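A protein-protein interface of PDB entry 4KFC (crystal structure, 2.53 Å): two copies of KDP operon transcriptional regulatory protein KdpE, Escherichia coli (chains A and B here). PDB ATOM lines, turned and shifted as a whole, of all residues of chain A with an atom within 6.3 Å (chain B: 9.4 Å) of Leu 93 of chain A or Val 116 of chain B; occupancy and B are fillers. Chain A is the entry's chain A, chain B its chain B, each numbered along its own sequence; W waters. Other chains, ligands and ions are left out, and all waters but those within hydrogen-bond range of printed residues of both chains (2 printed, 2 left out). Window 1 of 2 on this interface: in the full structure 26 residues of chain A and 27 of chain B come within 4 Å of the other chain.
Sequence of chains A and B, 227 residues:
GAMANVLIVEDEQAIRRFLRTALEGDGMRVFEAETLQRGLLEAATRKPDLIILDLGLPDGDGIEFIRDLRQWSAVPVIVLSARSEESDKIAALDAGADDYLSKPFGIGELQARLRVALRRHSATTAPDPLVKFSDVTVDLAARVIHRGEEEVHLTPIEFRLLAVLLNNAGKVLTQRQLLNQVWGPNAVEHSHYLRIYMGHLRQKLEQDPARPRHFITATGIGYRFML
The backbone carbonyl oxygen of Gly 96 of chain A sits close to the guanidinium group of Arg 119 of chain B (3.4 Å). The backbone carbonyl oxygen (O) of Tyr 100 of chain A sits at hydrogen-bond distance from the guanidinium group (NH2) of Arg 113 of chain B, at 3.2 Å. The side-chain carboxylate of Asp 99 of chain A is in salt-bridge range of the guanidinium group of Arg 113 of chain B, at 3.1 Å. The guanidinium group (NH1) of Arg 120 of chain B lies within salt-bridge range of the side-chain carboxylate (OD1) of Asp 98 of chain A, 3.3 Å away. The backbone carbonyl oxygen of Leu 93 of chain A is in hydrogen-bond range of the guanidinium group of Arg 119 of chain B, at 2.8 Å. O of Ala 97 of chain A is in hydrogen-bond range of NH2 of Arg 119 of chain B, at 2.6 Å. The side-chain carboxylate (OD2) of Asp 94 of chain A is in salt-bridge range of the guanidinium group (NH2) of Arg 115 of chain B (2.9 Å).
OD2 of Asp 26 of chain B lies within salt-bridge range of NH1 of Arg 115 of chain B, 3.1 Å away. The guanidinium group (NE) of Arg 113 of chain B lies within salt-bridge range of the side-chain carboxylate (OE2) of Glu 109 of chain B (2.9 Å). OD2 of Asp 88 of chain A lies within hydrogen-bond range of OH of Tyr 100 of chain A (2.9 Å). The guanidinium group (NH1) of Arg 113 of chain B lies within salt-bridge range of the side-chain carboxylate (OD2) of Asp 99 of chain B (3.0 Å). N of Ala 97 of chain A is in hydrogen-bond range of O of Ala 92 of chain A, 3.0 Å away.
Lys 89 of chain A touches Glu 109 of chain B (CD to CD, 3.5 Å). Ile 90 of chain A touches Gly 108 of chain B (CD1 to C, 3.8 Å). Leu 93 of chain A touches Ala 112 of chain B (CD1 to CB, 3.9 Å). Leu 93 of chain A touches Arg 113 of chain B (CD1 to CG, 3.8 Å). O of Leu 93 of chain A touches CG2 of Val 116 of chain B, at 3.9 Å. Val 116 of chain B touches Ala 97 of chain A (CG2 to O, 3.7 Å). Asp 98 of chain A touches Val 116 of chain B.
No residue of chain B comes within 4 Å of Ala 92 of chain A. Leu 93 of chain A touches just these residues of chain B: Ala 112, Arg 113, Val 116 and Arg 119. Asp 94 of chain A touches just one residue of chain B: Arg 115 (2.9 Å). No residue of chain B comes within 4 Å of Ala 95 of chain A. Printed residues of chain B within 4 Å of Gly 96 of chain A: Arg 119 (3.3 Å). Ala 97 of chain A touches just these residues of chain B: Val 116 and Arg 119. Asp 49 of chain B touches none of the printed residues of chain A. Of the printed residues of chain A, Ala 112 of chain B touches Leu 93. Of the printed residues of chain A, Val 116 of chain B touches Leu 93 (3.9 Å), Ala 97 (3.7 Å) and Asp 98 (3.6 Å). Printed residues of chain A within 4 Å of Arg 120 of chain B: Asp 98. The nearest printed residue of chain A that does not touch Arg 119 of chain B is Asp 94 of chain A (4.3 Å).
Among the printed residues, Asp or Glu carboxylates within 4 Å of a Lys or Arg side-chain nitrogen of the other chain: Asp 94 of chain A with Arg 115 of chain B (2.9 Å), Asp 98 of chain A with Arg 120 of chain B (3.3 Å) and Asp 99 of chain A with Arg 113 of chain B (3.1 Å).
2 positions are printed for both chains.
Water W2 bridges O of Asp 98 of chain A (2.6 Å) and NH1 of Arg 120 of chain B (3.1 Å). Water W1 lies within hydrogen-bond range of the backbone carbonyl oxygen of Asp 98 of chain A, the side-chain carboxylate of Asp 99 of chain B and the guanidinium group of Arg 113 of chain B.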
ATOM      1  N   ILE A  66       3.373 -17.680 -30.074  1.00  0.00           N
ATOM      2  CA  ILE A  66       3.161 -18.049 -28.683  1.00  0.00           C
ATOM      3  C   ILE A  66       2.806 -16.843 -27.815  1.00  0.00           C
ATOM      4  O   ILE A  66       1.846 -16.898 -27.051  1.00  0.00           O
ATOM      5  CB  ILE A  66       4.389 -18.764 -28.107  1.00  0.00           C
ATOM      6  CG1 ILE A  66       4.557 -20.125 -28.782  1.00  0.00           C
ATOM      7  CG2 ILE A  66       4.262 -18.915 -26.603  1.00  0.00           C
ATOM      8  CD1 ILE A  66       5.752 -20.902 -28.288  1.00  0.00           C
ATOM      9  N   ASP A  88      16.965 -22.298 -27.949  1.00  0.00           N
ATOM     10  CA  ASP A  88      15.642 -22.256 -28.570  1.00  0.00           C
ATOM     11  C   ASP A  88      14.581 -22.868 -27.655  1.00  0.00           C
ATOM     12  O   ASP A  88      13.459 -22.356 -27.564  1.00  0.00           O
ATOM     13  CB  ASP A  88      15.661 -22.968 -29.924  1.00  0.00           C
ATOM     14  CG  ASP A  88      14.374 -22.769 -30.708  1.00  0.00           C
ATOM     15  OD1 ASP A  88      13.691 -21.742 -30.486  1.00  0.00           O
ATOM     16  OD2 ASP A  88      14.049 -23.639 -31.549  1.00  0.00           O
ATOM     17  N   LYS A  89      14.945 -23.961 -26.983  1.00  0.00           N
ATOM     18  CA  LYS A  89      14.082 -24.571 -25.979  1.00  0.00           C
ATOM     19  C   LYS A  89      13.707 -23.532 -24.937  1.00  0.00           C
ATOM     20  O   LYS A  89      12.527 -23.288 -24.686  1.00  0.00           O
ATOM     21  CB  LYS A  89      14.785 -25.736 -25.275  1.00  0.00           C
ATOM     22  CG  LYS A  89      15.023 -26.975 -26.124  1.00  0.00           C
ATOM     23  CD  LYS A  89      15.161 -28.211 -25.233  1.00  0.00           C
ATOM     24  CE  LYS A  89      15.390 -29.484 -26.041  1.00  0.00           C
ATOM     25  NZ  LYS A  89      16.724 -29.496 -26.703  1.00  0.00           N
ATOM     26  N   ILE A  90      14.726 -22.925 -24.336  1.00  0.00           N
ATOM     27  CA  ILE A  90      14.520 -21.933 -23.289  1.00  0.00           C
ATOM     28  C   ILE A  90      13.638 -20.788 -23.781  1.00  0.00           C
ATOM     29  O   ILE A  90      12.687 -20.400 -23.108  1.00  0.00           O
ATOM     30  CB  ILE A  90      15.859 -21.390 -22.764  1.00  0.00           C
ATOM     31  CG1 ILE A  90      16.666 -22.525 -22.128  1.00  0.00           C
ATOM     32  CG2 ILE A  90      15.626 -20.276 -21.754  1.00  0.00           C
ATOM     33  CD1 ILE A  90      18.101 -22.170 -21.826  1.00  0.00           C
ATOM     34  N   ALA A  91      13.949 -20.272 -24.966  1.00  0.00           N
ATOM     35  CA  ALA A  91      13.182 -19.186 -25.563  1.00  0.00           C
ATOM     36  C   ALA A  91      11.698 -19.542 -25.707  1.00  0.00           C
ATOM     37  O   ALA A  91      10.827 -18.763 -25.302  1.00  0.00           O
ATOM     38  CB  ALA A  91      13.776 -18.809 -26.909  1.00  0.00           C
ATOM     39  N   ALA A  92      11.415 -20.718 -26.267  1.00  0.00           N
ATOM     40  CA  ALA A  92      10.031 -21.167 -26.460  1.00  0.00           C
ATOM     41  C   ALA A  92       9.290 -21.397 -25.141  1.00  0.00           C
ATOM     42  O   ALA A  92       8.125 -21.018 -24.999  1.00  0.00           O
ATOM     43  CB  ALA A  92       9.999 -22.418 -27.298  1.00  0.00           C
ATOM     44  N   LEU A  93       9.964 -22.030 -24.187  1.00  0.00           N
ATOM     45  CA  LEU A  93       9.365 -22.319 -22.889  1.00  0.00           C
ATOM     46  C   LEU A  93       9.069 -21.038 -22.109  1.00  0.00           C
ATOM     47  O   LEU A  93       8.036 -20.927 -21.449  1.00  0.00           O
ATOM     48  CB  LEU A  93      10.278 -23.232 -22.068  1.00  0.00           C
ATOM     49  CG  LEU A  93      10.422 -24.660 -22.588  1.00  0.00           C
ATOM     50  CD1 LEU A  93      11.356 -25.466 -21.703  1.00  0.00           C
ATOM     51  CD2 LEU A  93       9.056 -25.316 -22.658  1.00  0.00           C
ATOM     52  N   ASP A  94       9.977 -20.073 -22.189  1.00  0.00           N
ATOM     53  CA  ASP A  94       9.806 -18.819 -21.467  1.00  0.00           C
ATOM     54  C   ASP A  94       8.786 -17.931 -22.169  1.00  0.00           C
ATOM     55  O   ASP A  94       8.130 -17.108 -21.535  1.00  0.00           O
ATOM     56  CB  ASP A  94      11.149 -18.098 -21.294  1.00  0.00           C
ATOM     57  CG  ASP A  94      12.059 -18.783 -20.271  1.00  0.00           C
ATOM     58  OD1 ASP A  94      11.552 -19.592 -19.465  1.00  0.00           O
ATOM     59  OD2 ASP A  94      13.278 -18.502 -20.264  1.00  0.00           O
ATOM     60  N   ALA A  95       8.648 -18.112 -23.480  1.00  0.00           N
ATOM     61  CA  ALA A  95       7.626 -17.401 -24.244  1.00  0.00           C
ATOM     62  C   ALA A  95       6.226 -17.826 -23.805  1.00  0.00           C
ATOM     63  O   ALA A  95       5.281 -17.039 -23.862  1.00  0.00           O
ATOM     64  CB  ALA A  95       7.808 -17.644 -25.731  1.00  0.00           C
ATOM     65  N   GLY A  96       6.089 -19.078 -23.378  1.00  0.00           N
ATOM     66  CA  GLY A  96       4.812 -19.556 -22.884  1.00  0.00           C
ATOM     67  C   GLY A  96       4.461 -20.979 -23.279  1.00  0.00           C
ATOM     68  O   GLY A  96       3.364 -21.453 -22.984  1.00  0.00           O
ATOM     69  N   ALA A  97       5.380 -21.667 -23.946  1.00  0.00           N
ATOM     70  CA  ALA A  97       5.136 -23.062 -24.298  1.00  0.00           C
ATOM     71  C   ALA A  97       5.178 -23.937 -23.046  1.00  0.00           C
ATOM     72  O   ALA A  97       5.816 -23.587 -22.052  1.00  0.00           O
ATOM     73  CB  ALA A  97       6.134 -23.548 -25.321  1.00  0.00           C
ATOM     74  N   ASP A  98       4.506 -25.079 -23.104  1.00  0.00           N
ATOM     75  CA  ASP A  98       4.402 -25.959 -21.950  1.00  0.00           C
ATOM     76  C   ASP A  98       5.328 -27.154 -22.093  1.00  0.00           C
ATOM     77  O   ASP A  98       5.702 -27.789 -21.102  1.00  0.00           O
ATOM     78  CB  ASP A  98       2.960 -26.433 -21.788  1.00  0.00           C
ATOM     79  CG  ASP A  98       2.014 -25.300 -21.441  1.00  0.00           C
ATOM     80  OD1 ASP A  98       1.674 -25.148 -20.247  1.00  0.00           O
ATOM     81  OD2 ASP A  98       1.620 -24.553 -22.363  1.00  0.00           O
ATOM     82  N   ASP A  99       5.689 -27.456 -23.337  1.00  0.00           N
ATOM     83  CA  ASP A  99       6.575 -28.569 -23.633  1.00  0.00           C
ATOM     84  C   ASP A  99       7.279 -28.349 -24.966  1.00  0.00           C
ATOM     85  O   ASP A  99       6.839 -27.538 -25.794  1.00  0.00           O
ATOM     86  CB  ASP A  99       5.800 -29.890 -23.647  1.00  0.00           C
ATOM     87  CG  ASP A  99       6.646 -31.063 -23.174  1.00  0.00           C
ATOM     88  OD1 ASP A  99       7.890 -30.984 -23.283  1.00  0.00           O
ATOM     89  OD2 ASP A  99       6.070 -32.058 -22.684  1.00  0.00           O
ATOM     90  N   TYR A 100       8.368 -29.083 -25.169  1.00  0.00           N
ATOM     91  CA  TYR A 100       9.220 -28.908 -26.340  1.00  0.00           C
ATOM     92  C   TYR A 100       9.856 -30.243 -26.731  1.00  0.00           C
ATOM     93  O   TYR A 100      10.561 -30.865 -25.935  1.00  0.00           O
ATOM     94  CB  TYR A 100      10.308 -27.888 -26.017  1.00  0.00           C
ATOM     95  CG  TYR A 100      11.179 -27.452 -27.173  1.00  0.00           C
ATOM     96  CD1 TYR A 100      12.132 -28.301 -27.721  1.00  0.00           C
ATOM     97  CD2 TYR A 100      11.084 -26.165 -27.681  1.00  0.00           C
ATOM     98  CE1 TYR A 100      12.940 -27.892 -28.768  1.00  0.00           C
ATOM     99  CE2 TYR A 100      11.891 -25.743 -28.723  1.00  0.00           C
ATOM    100  CZ  TYR A 100      12.817 -26.612 -29.261  1.00  0.00           C
ATOM    101  OH  TYR A 100      13.625 -26.199 -30.294  1.00  0.00           O
ATOM    102  N   ASP B  26      18.307 -20.022  -9.515  1.00  0.00           N
ATOM    103  CA  ASP B  26      17.063 -19.416  -9.987  1.00  0.00           C
ATOM    104  C   ASP B  26      16.114 -19.055  -8.841  1.00  0.00           C
ATOM    105  O   ASP B  26      14.899 -18.985  -9.033  1.00  0.00           O
ATOM    106  CB  ASP B  26      16.361 -20.338 -10.993  1.00  0.00           C
ATOM    107  CG  ASP B  26      15.615 -19.567 -12.071  1.00  0.00           C
ATOM    108  OD1 ASP B  26      16.042 -18.438 -12.397  1.00  0.00           O
ATOM    109  OD2 ASP B  26      14.607 -20.091 -12.595  1.00  0.00           O
ATOM    110  N   MET B  28      15.259 -20.526  -5.726  1.00  0.00           N
ATOM    111  CA  MET B  28      14.364 -21.483  -5.085  1.00  0.00           C
ATOM    112  C   MET B  28      15.014 -22.110  -3.855  1.00  0.00           C
ATOM    113  O   MET B  28      16.219 -22.363  -3.847  1.00  0.00           O
ATOM    114  CB  MET B  28      13.941 -22.562  -6.086  1.00  0.00           C
ATOM    115  CG  MET B  28      13.430 -21.993  -7.409  1.00  0.00           C
ATOM    116  SD  MET B  28      12.906 -23.239  -8.605  1.00  0.00           S
ATOM    117  CE  MET B  28      12.758 -22.248 -10.097  1.00  0.00           C
ATOM    118  N   ASP B  49       6.491 -27.009  -3.513  1.00  0.00           N
ATOM    119  CA  ASP B  49       5.777 -26.498  -4.667  1.00  0.00           C
ATOM    120  C   ASP B  49       6.104 -27.327  -5.900  1.00  0.00           C
ATOM    121  O   ASP B  49       5.396 -27.268  -6.904  1.00  0.00           O
ATOM    122  CB  ASP B  49       6.130 -25.032  -4.895  1.00  0.00           C
ATOM    123  CG  ASP B  49       5.812 -24.171  -3.690  1.00  0.00           C
ATOM    124  OD1 ASP B  49       4.611 -24.011  -3.381  1.00  0.00           O
ATOM    125  OD2 ASP B  49       6.759 -23.665  -3.047  1.00  0.00           O
ATOM    126  N   LEU B  50       7.172 -28.113  -5.804  1.00  0.00           N
ATOM    127  CA  LEU B  50       7.623 -28.947  -6.906  1.00  0.00           C
ATOM    128  C   LEU B  50       8.541 -30.049  -6.387  1.00  0.00           C
ATOM    129  O   LEU B  50       9.306 -29.839  -5.439  1.00  0.00           O
ATOM    130  CB  LEU B  50       8.347 -28.092  -7.946  1.00  0.00           C
ATOM    131  CG  LEU B  50       8.559 -28.699  -9.333  1.00  0.00           C
ATOM    132  CD1 LEU B  50       8.589 -27.601 -10.371  1.00  0.00           C
ATOM    133  CD2 LEU B  50       9.850 -29.476  -9.391  1.00  0.00           C
ATOM    134  N   PRO B  76       3.439 -30.738  -8.725  1.00  0.00           N
ATOM    135  CA  PRO B  76       4.171 -31.007  -9.970  1.00  0.00           C
ATOM    136  C   PRO B  76       5.414 -31.869  -9.731  1.00  0.00           C
ATOM    137  O   PRO B  76       6.203 -31.584  -8.823  1.00  0.00           O
ATOM    138  CB  PRO B  76       4.586 -29.609 -10.451  1.00  0.00           C
ATOM    139  CG  PRO B  76       3.575 -28.676  -9.826  1.00  0.00           C
ATOM    140  CD  PRO B  76       3.213 -29.296  -8.505  1.00  0.00           C
ATOM    141  N   ILE B  78       8.827 -33.383 -11.643  1.00  0.00           N
ATOM    142  CA  ILE B  78       9.739 -33.431 -12.773  1.00  0.00           C
ATOM    143  C   ILE B  78      10.656 -34.629 -12.573  1.00  0.00           C
ATOM    144  O   ILE B  78      11.347 -34.737 -11.558  1.00  0.00           O
ATOM    145  CB  ILE B  78      10.570 -32.150 -12.898  1.00  0.00           C
ATOM    146  CG1 ILE B  78       9.667 -30.967 -13.233  1.00  0.00           C
ATOM    147  CG2 ILE B  78      11.638 -32.304 -13.972  1.00  0.00           C
ATOM    148  CD1 ILE B  78      10.434 -29.719 -13.580  1.00  0.00           C
ATOM    149  N   ASP B  98       4.889 -34.734 -14.545  1.00  0.00           N
ATOM    150  CA  ASP B  98       4.502 -33.614 -15.399  1.00  0.00           C
ATOM    151  C   ASP B  98       5.540 -33.351 -16.468  1.00  0.00           C
ATOM    152  O   ASP B  98       5.228 -32.795 -17.526  1.00  0.00           O
ATOM    153  CB  ASP B  98       4.303 -32.341 -14.577  1.00  0.00           C
ATOM    154  CG  ASP B  98       3.144 -32.446 -13.615  1.00  0.00           C
ATOM    155  OD1 ASP B  98       1.994 -32.183 -14.034  1.00  0.00           O
ATOM    156  OD2 ASP B  98       3.388 -32.788 -12.437  1.00  0.00           O
ATOM    157  N   ASP B  99       6.779 -33.734 -16.180  1.00  0.00           N
ATOM    158  CA  ASP B  99       7.846 -33.612 -17.157  1.00  0.00           C
ATOM    159  C   ASP B  99       8.890 -34.703 -16.960  1.00  0.00           C
ATOM    160  O   ASP B  99       8.939 -35.351 -15.906  1.00  0.00           O
ATOM    161  CB  ASP B  99       8.490 -32.226 -17.094  1.00  0.00           C
ATOM    162  CG  ASP B  99       9.128 -31.827 -18.410  1.00  0.00           C
ATOM    163  OD1 ASP B  99       9.328 -32.717 -19.266  1.00  0.00           O
ATOM    164  OD2 ASP B  99       9.430 -30.629 -18.593  1.00  0.00           O
ATOM    165  N   LEU B 101      13.085 -35.526 -18.095  1.00  0.00           N
ATOM    166  CA  LEU B 101      14.338 -35.082 -18.685  1.00  0.00           C
ATOM    167  C   LEU B 101      15.305 -36.255 -18.807  1.00  0.00           C
ATOM    168  O   LEU B 101      15.531 -36.995 -17.834  1.00  0.00           O
ATOM    169  CB  LEU B 101      14.973 -33.983 -17.830  1.00  0.00           C
ATOM    170  CG  LEU B 101      14.433 -32.555 -17.930  1.00  0.00           C
ATOM    171  CD1 LEU B 101      13.013 -32.452 -17.404  1.00  0.00           C
ATOM    172  CD2 LEU B 101      15.342 -31.600 -17.176  1.00  0.00           C
ATOM    173  N   GLY B 108      20.287 -24.649 -17.912  1.00  0.00           N
ATOM    174  CA  GLY B 108      19.331 -23.741 -18.524  1.00  0.00           C
ATOM    175  C   GLY B 108      17.973 -24.371 -18.775  1.00  0.00           C
ATOM    176  O   GLY B 108      16.947 -23.861 -18.306  1.00  0.00           O
ATOM    177  N   GLU B 109      17.968 -25.485 -19.503  1.00  0.00           N
ATOM    178  CA  GLU B 109      16.727 -26.171 -19.826  1.00  0.00           C
ATOM    179  C   GLU B 109      16.002 -26.626 -18.564  1.00  0.00           C
ATOM    180  O   GLU B 109      14.780 -26.502 -18.472  1.00  0.00           O
ATOM    181  CB  GLU B 109      16.977 -27.362 -20.756  1.00  0.00           C
ATOM    182  CG  GLU B 109      15.690 -28.010 -21.271  1.00  0.00           C
ATOM    183  CD  GLU B 109      15.928 -29.325 -21.997  1.00  0.00           C
ATOM    184  OE1 GLU B 109      17.086 -29.597 -22.389  1.00  0.00           O
ATOM    185  OE2 GLU B 109      14.950 -30.087 -22.174  1.00  0.00           O
ATOM    186  N   LEU B 110      16.751 -27.146 -17.593  1.00  0.00           N
ATOM    187  CA  LEU B 110      16.143 -27.600 -16.345  1.00  0.00           C
ATOM    188  C   LEU B 110      15.453 -26.442 -15.631  1.00  0.00           C
ATOM    189  O   LEU B 110      14.327 -26.585 -15.151  1.00  0.00           O
ATOM    190  CB  LEU B 110      17.172 -28.265 -15.425  1.00  0.00           C
ATOM    191  CG  LEU B 110      16.665 -28.600 -14.015  1.00  0.00           C
ATOM    192  CD1 LEU B 110      15.427 -29.484 -14.058  1.00  0.00           C
ATOM    193  CD2 LEU B 110      17.749 -29.258 -13.192  1.00  0.00           C
ATOM    194  N   GLN B 111      16.124 -25.294 -15.581  1.00  0.00           N
ATOM    195  CA  GLN B 111      15.533 -24.102 -14.980  1.00  0.00           C
ATOM    196  C   GLN B 111      14.265 -23.663 -15.723  1.00  0.00           C
ATOM    197  O   GLN B 111      13.257 -23.325 -15.098  1.00  0.00           O
ATOM    198  CB  GLN B 111      16.558 -22.966 -14.917  1.00  0.00           C
ATOM    199  CG  GLN B 111      17.607 -23.148 -13.817  1.00  0.00           C
ATOM    200  CD  GLN B 111      18.824 -22.255 -14.004  1.00  0.00           C
ATOM    201  OE1 GLN B 111      19.101 -21.782 -15.107  1.00  0.00           O
ATOM    202  NE2 GLN B 111      19.562 -22.028 -12.922  1.00  0.00           N
ATOM    203  N   ALA B 112      14.313 -23.682 -17.053  1.00  0.00           N
ATOM    204  CA  ALA B 112      13.144 -23.322 -17.857  1.00  0.00           C
ATOM    205  C   ALA B 112      11.941 -24.249 -17.592  1.00  0.00           C
ATOM    206  O   ALA B 112      10.812 -23.785 -17.409  1.00  0.00           O
ATOM    207  CB  ALA B 112      13.495 -23.297 -19.329  1.00  0.00           C
ATOM    208  N   ARG B 113      12.191 -25.554 -17.551  1.00  0.00           N
ATOM    209  CA  ARG B 113      11.122 -26.520 -17.300  1.00  0.00           C
ATOM    210  C   ARG B 113      10.605 -26.422 -15.867  1.00  0.00           C
ATOM    211  O   ARG B 113       9.431 -26.697 -15.594  1.00  0.00           O
ATOM    212  CB  ARG B 113      11.588 -27.944 -17.627  1.00  0.00           C
ATOM    213  CG  ARG B 113      12.080 -28.097 -19.067  1.00  0.00           C
ATOM    214  CD  ARG B 113      12.188 -29.545 -19.503  1.00  0.00           C
ATOM    215  NE  ARG B 113      12.410 -29.646 -20.944  1.00  0.00           N
ATOM    216  CZ  ARG B 113      11.445 -29.842 -21.839  1.00  0.00           C
ATOM    217  NH1 ARG B 113      10.185 -29.980 -21.447  1.00  0.00           N
ATOM    218  NH2 ARG B 113      11.740 -29.909 -23.131  1.00  0.00           N
ATOM    219  N   LEU B 114      11.482 -26.012 -14.959  1.00  0.00           N
ATOM    220  CA  LEU B 114      11.079 -25.728 -13.585  1.00  0.00           C
ATOM    221  C   LEU B 114      10.119 -24.537 -13.539  1.00  0.00           C
ATOM    222  O   LEU B 114       9.065 -24.603 -12.898  1.00  0.00           O
ATOM    223  CB  LEU B 114      12.309 -25.458 -12.716  1.00  0.00           C
ATOM    224  CG  LEU B 114      13.011 -26.720 -12.225  1.00  0.00           C
ATOM    225  CD1 LEU B 114      14.423 -26.426 -11.746  1.00  0.00           C
ATOM    226  CD2 LEU B 114      12.192 -27.327 -11.109  1.00  0.00           C
ATOM    227  N   ARG B 115      10.479 -23.455 -14.231  1.00  0.00           N
ATOM    228  CA  ARG B 115       9.610 -22.281 -14.306  1.00  0.00           C
ATOM    229  C   ARG B 115       8.264 -22.653 -14.922  1.00  0.00           C
ATOM    230  O   ARG B 115       7.216 -22.246 -14.420  1.00  0.00           O
ATOM    231  CB  ARG B 115      10.263 -21.145 -15.102  1.00  0.00           C
ATOM    232  CG  ARG B 115      11.410 -20.450 -14.374  1.00  0.00           C
ATOM    233  CD  ARG B 115      11.895 -19.209 -15.130  1.00  0.00           C
ATOM    234  NE  ARG B 115      12.452 -19.515 -16.447  1.00  0.00           N
ATOM    235  CZ  ARG B 115      13.736 -19.775 -16.679  1.00  0.00           C
ATOM    236  NH1 ARG B 115      14.609 -19.779 -15.681  1.00  0.00           N
ATOM    237  NH2 ARG B 115      14.150 -20.033 -17.909  1.00  0.00           N
ATOM    238  N   VAL B 116       8.297 -23.437 -15.998  1.00  0.00           N
ATOM    239  CA  VAL B 116       7.070 -23.907 -16.634  1.00  0.00           C
ATOM    240  C   VAL B 116       6.194 -24.656 -15.637  1.00  0.00           C
ATOM    241  O   VAL B 116       5.007 -24.369 -15.502  1.00  0.00           O
ATOM    242  CB  VAL B 116       7.356 -24.805 -17.856  1.00  0.00           C
ATOM    243  CG1 VAL B 116       6.117 -25.598 -18.241  1.00  0.00           C
ATOM    244  CG2 VAL B 116       7.840 -23.961 -19.037  1.00  0.00           C
ATOM    245  N   ALA B 117       6.785 -25.599 -14.918  1.00  0.00           N
ATOM    246  CA  ALA B 117       6.009 -26.394 -13.973  1.00  0.00           C
ATOM    247  C   ALA B 117       5.462 -25.565 -12.806  1.00  0.00           C
ATOM    248  O   ALA B 117       4.388 -25.860 -12.285  1.00  0.00           O
ATOM    249  CB  ALA B 117       6.830 -27.568 -13.463  1.00  0.00           C
ATOM    250  N   LEU B 118       6.195 -24.525 -12.410  1.00  0.00           N
ATOM    251  CA  LEU B 118       5.812 -23.697 -11.262  1.00  0.00           C
ATOM    252  C   LEU B 118       4.791 -22.593 -11.569  1.00  0.00           C
ATOM    253  O   LEU B 118       3.994 -22.231 -10.705  1.00  0.00           O
ATOM    254  CB  LEU B 118       7.053 -23.085 -10.603  1.00  0.00           C
ATOM    255  CG  LEU B 118       7.909 -24.071  -9.809  1.00  0.00           C
ATOM    256  CD1 LEU B 118       9.253 -23.471  -9.431  1.00  0.00           C
ATOM    257  CD2 LEU B 118       7.154 -24.505  -8.574  1.00  0.00           C
ATOM    258  N   ARG B 119       4.807 -22.064 -12.790  1.00  0.00           N
ATOM    259  CA  ARG B 119       3.948 -20.926 -13.131  1.00  0.00           C
ATOM    260  C   ARG B 119       2.471 -21.283 -13.260  1.00  0.00           C
ATOM    261  O   ARG B 119       1.627 -20.401 -13.413  1.00  0.00           O
ATOM    262  CB  ARG B 119       4.432 -20.231 -14.409  1.00  0.00           C
ATOM    263  CG  ARG B 119       4.147 -20.987 -15.699  1.00  0.00           C
ATOM    264  CD  ARG B 119       4.927 -20.364 -16.848  1.00  0.00           C
ATOM    265  NE  ARG B 119       4.732 -21.071 -18.111  1.00  0.00           N
ATOM    266  CZ  ARG B 119       5.626 -21.094 -19.097  1.00  0.00           C
ATOM    267  NH1 ARG B 119       6.783 -20.459 -18.960  1.00  0.00           N
ATOM    268  NH2 ARG B 119       5.367 -21.761 -20.213  1.00  0.00           N
ATOM    269  N   ARG B 120       2.159 -22.574 -13.194  1.00  0.00           N
ATOM    270  CA  ARG B 120       0.774 -23.020 -13.267  1.00  0.00           C
ATOM    271  C   ARG B 120       0.048 -22.870 -11.932  1.00  0.00           C
ATOM    272  O   ARG B 120      -1.154 -22.605 -11.897  1.00  0.00           O
ATOM    273  CB  ARG B 120       0.693 -24.456 -13.788  1.00  0.00           C
ATOM    274  CG  ARG B 120       0.920 -24.558 -15.289  1.00  0.00           C
ATOM    275  CD  ARG B 120       0.657 -25.956 -15.798  1.00  0.00           C
ATOM    276  NE  ARG B 120       1.749 -26.865 -15.469  1.00  0.00           N
ATOM    277  CZ  ARG B 120       2.616 -27.345 -16.355  1.00  0.00           C
ATOM    278  NH1 ARG B 120       2.511 -27.011 -17.638  1.00  0.00           N
ATOM    279  NH2 ARG B 120       3.580 -28.169 -15.960  1.00  0.00           N
ATOM    280  N   HIS B 121       0.779 -23.029 -10.835  1.00  0.00           N
ATOM    281  CA  HIS B 121       0.210 -22.825  -9.508  1.00  0.00           C
ATOM    282  C   HIS B 121       0.711 -21.515  -8.896  1.00  0.00           C
ATOM    283  O   HIS B 121       1.374 -21.524  -7.857  1.00  0.00           O
ATOM    284  CB  HIS B 121       0.545 -24.001  -8.584  1.00  0.00           C
ATOM    285  CG  HIS B 121      -0.071 -25.303  -9.001  1.00  0.00           C
ATOM    286  ND1 HIS B 121      -1.368 -25.654  -8.665  1.00  0.00           N
ATOM    287  CD2 HIS B 121       0.428 -26.340  -9.703  1.00  0.00           C
ATOM    288  CE1 HIS B 121      -1.632 -26.848  -9.154  1.00  0.00           C
ATOM    289  NE2 HIS B 121      -0.564 -27.294  -9.790  1.00  0.00           N
ATOM    290  N   SER B 122       0.395 -20.394  -9.543  1.00  0.00           N
ATOM    291  CA  SER B 122       0.813 -19.078  -9.056  1.00  0.00           C
ATOM    292  C   SER B 122      -0.024 -17.946  -9.645  1.00  0.00           C
ATOM    293  O   SER B 122       0.262 -16.769  -9.419  1.00  0.00           O
ATOM    294  CB  SER B 122       2.296 -18.834  -9.350  1.00  0.00           C
ATOM    295  OG  SER B 122       3.118 -19.686  -8.573  1.00  0.00           O
HETATM  296  O   HOH W   1       8.114 -28.418 -19.976  1.00  0.00           O
HETATM  297  O   HOH W   2       4.206 -28.974 -19.275  1.00  0.00           O
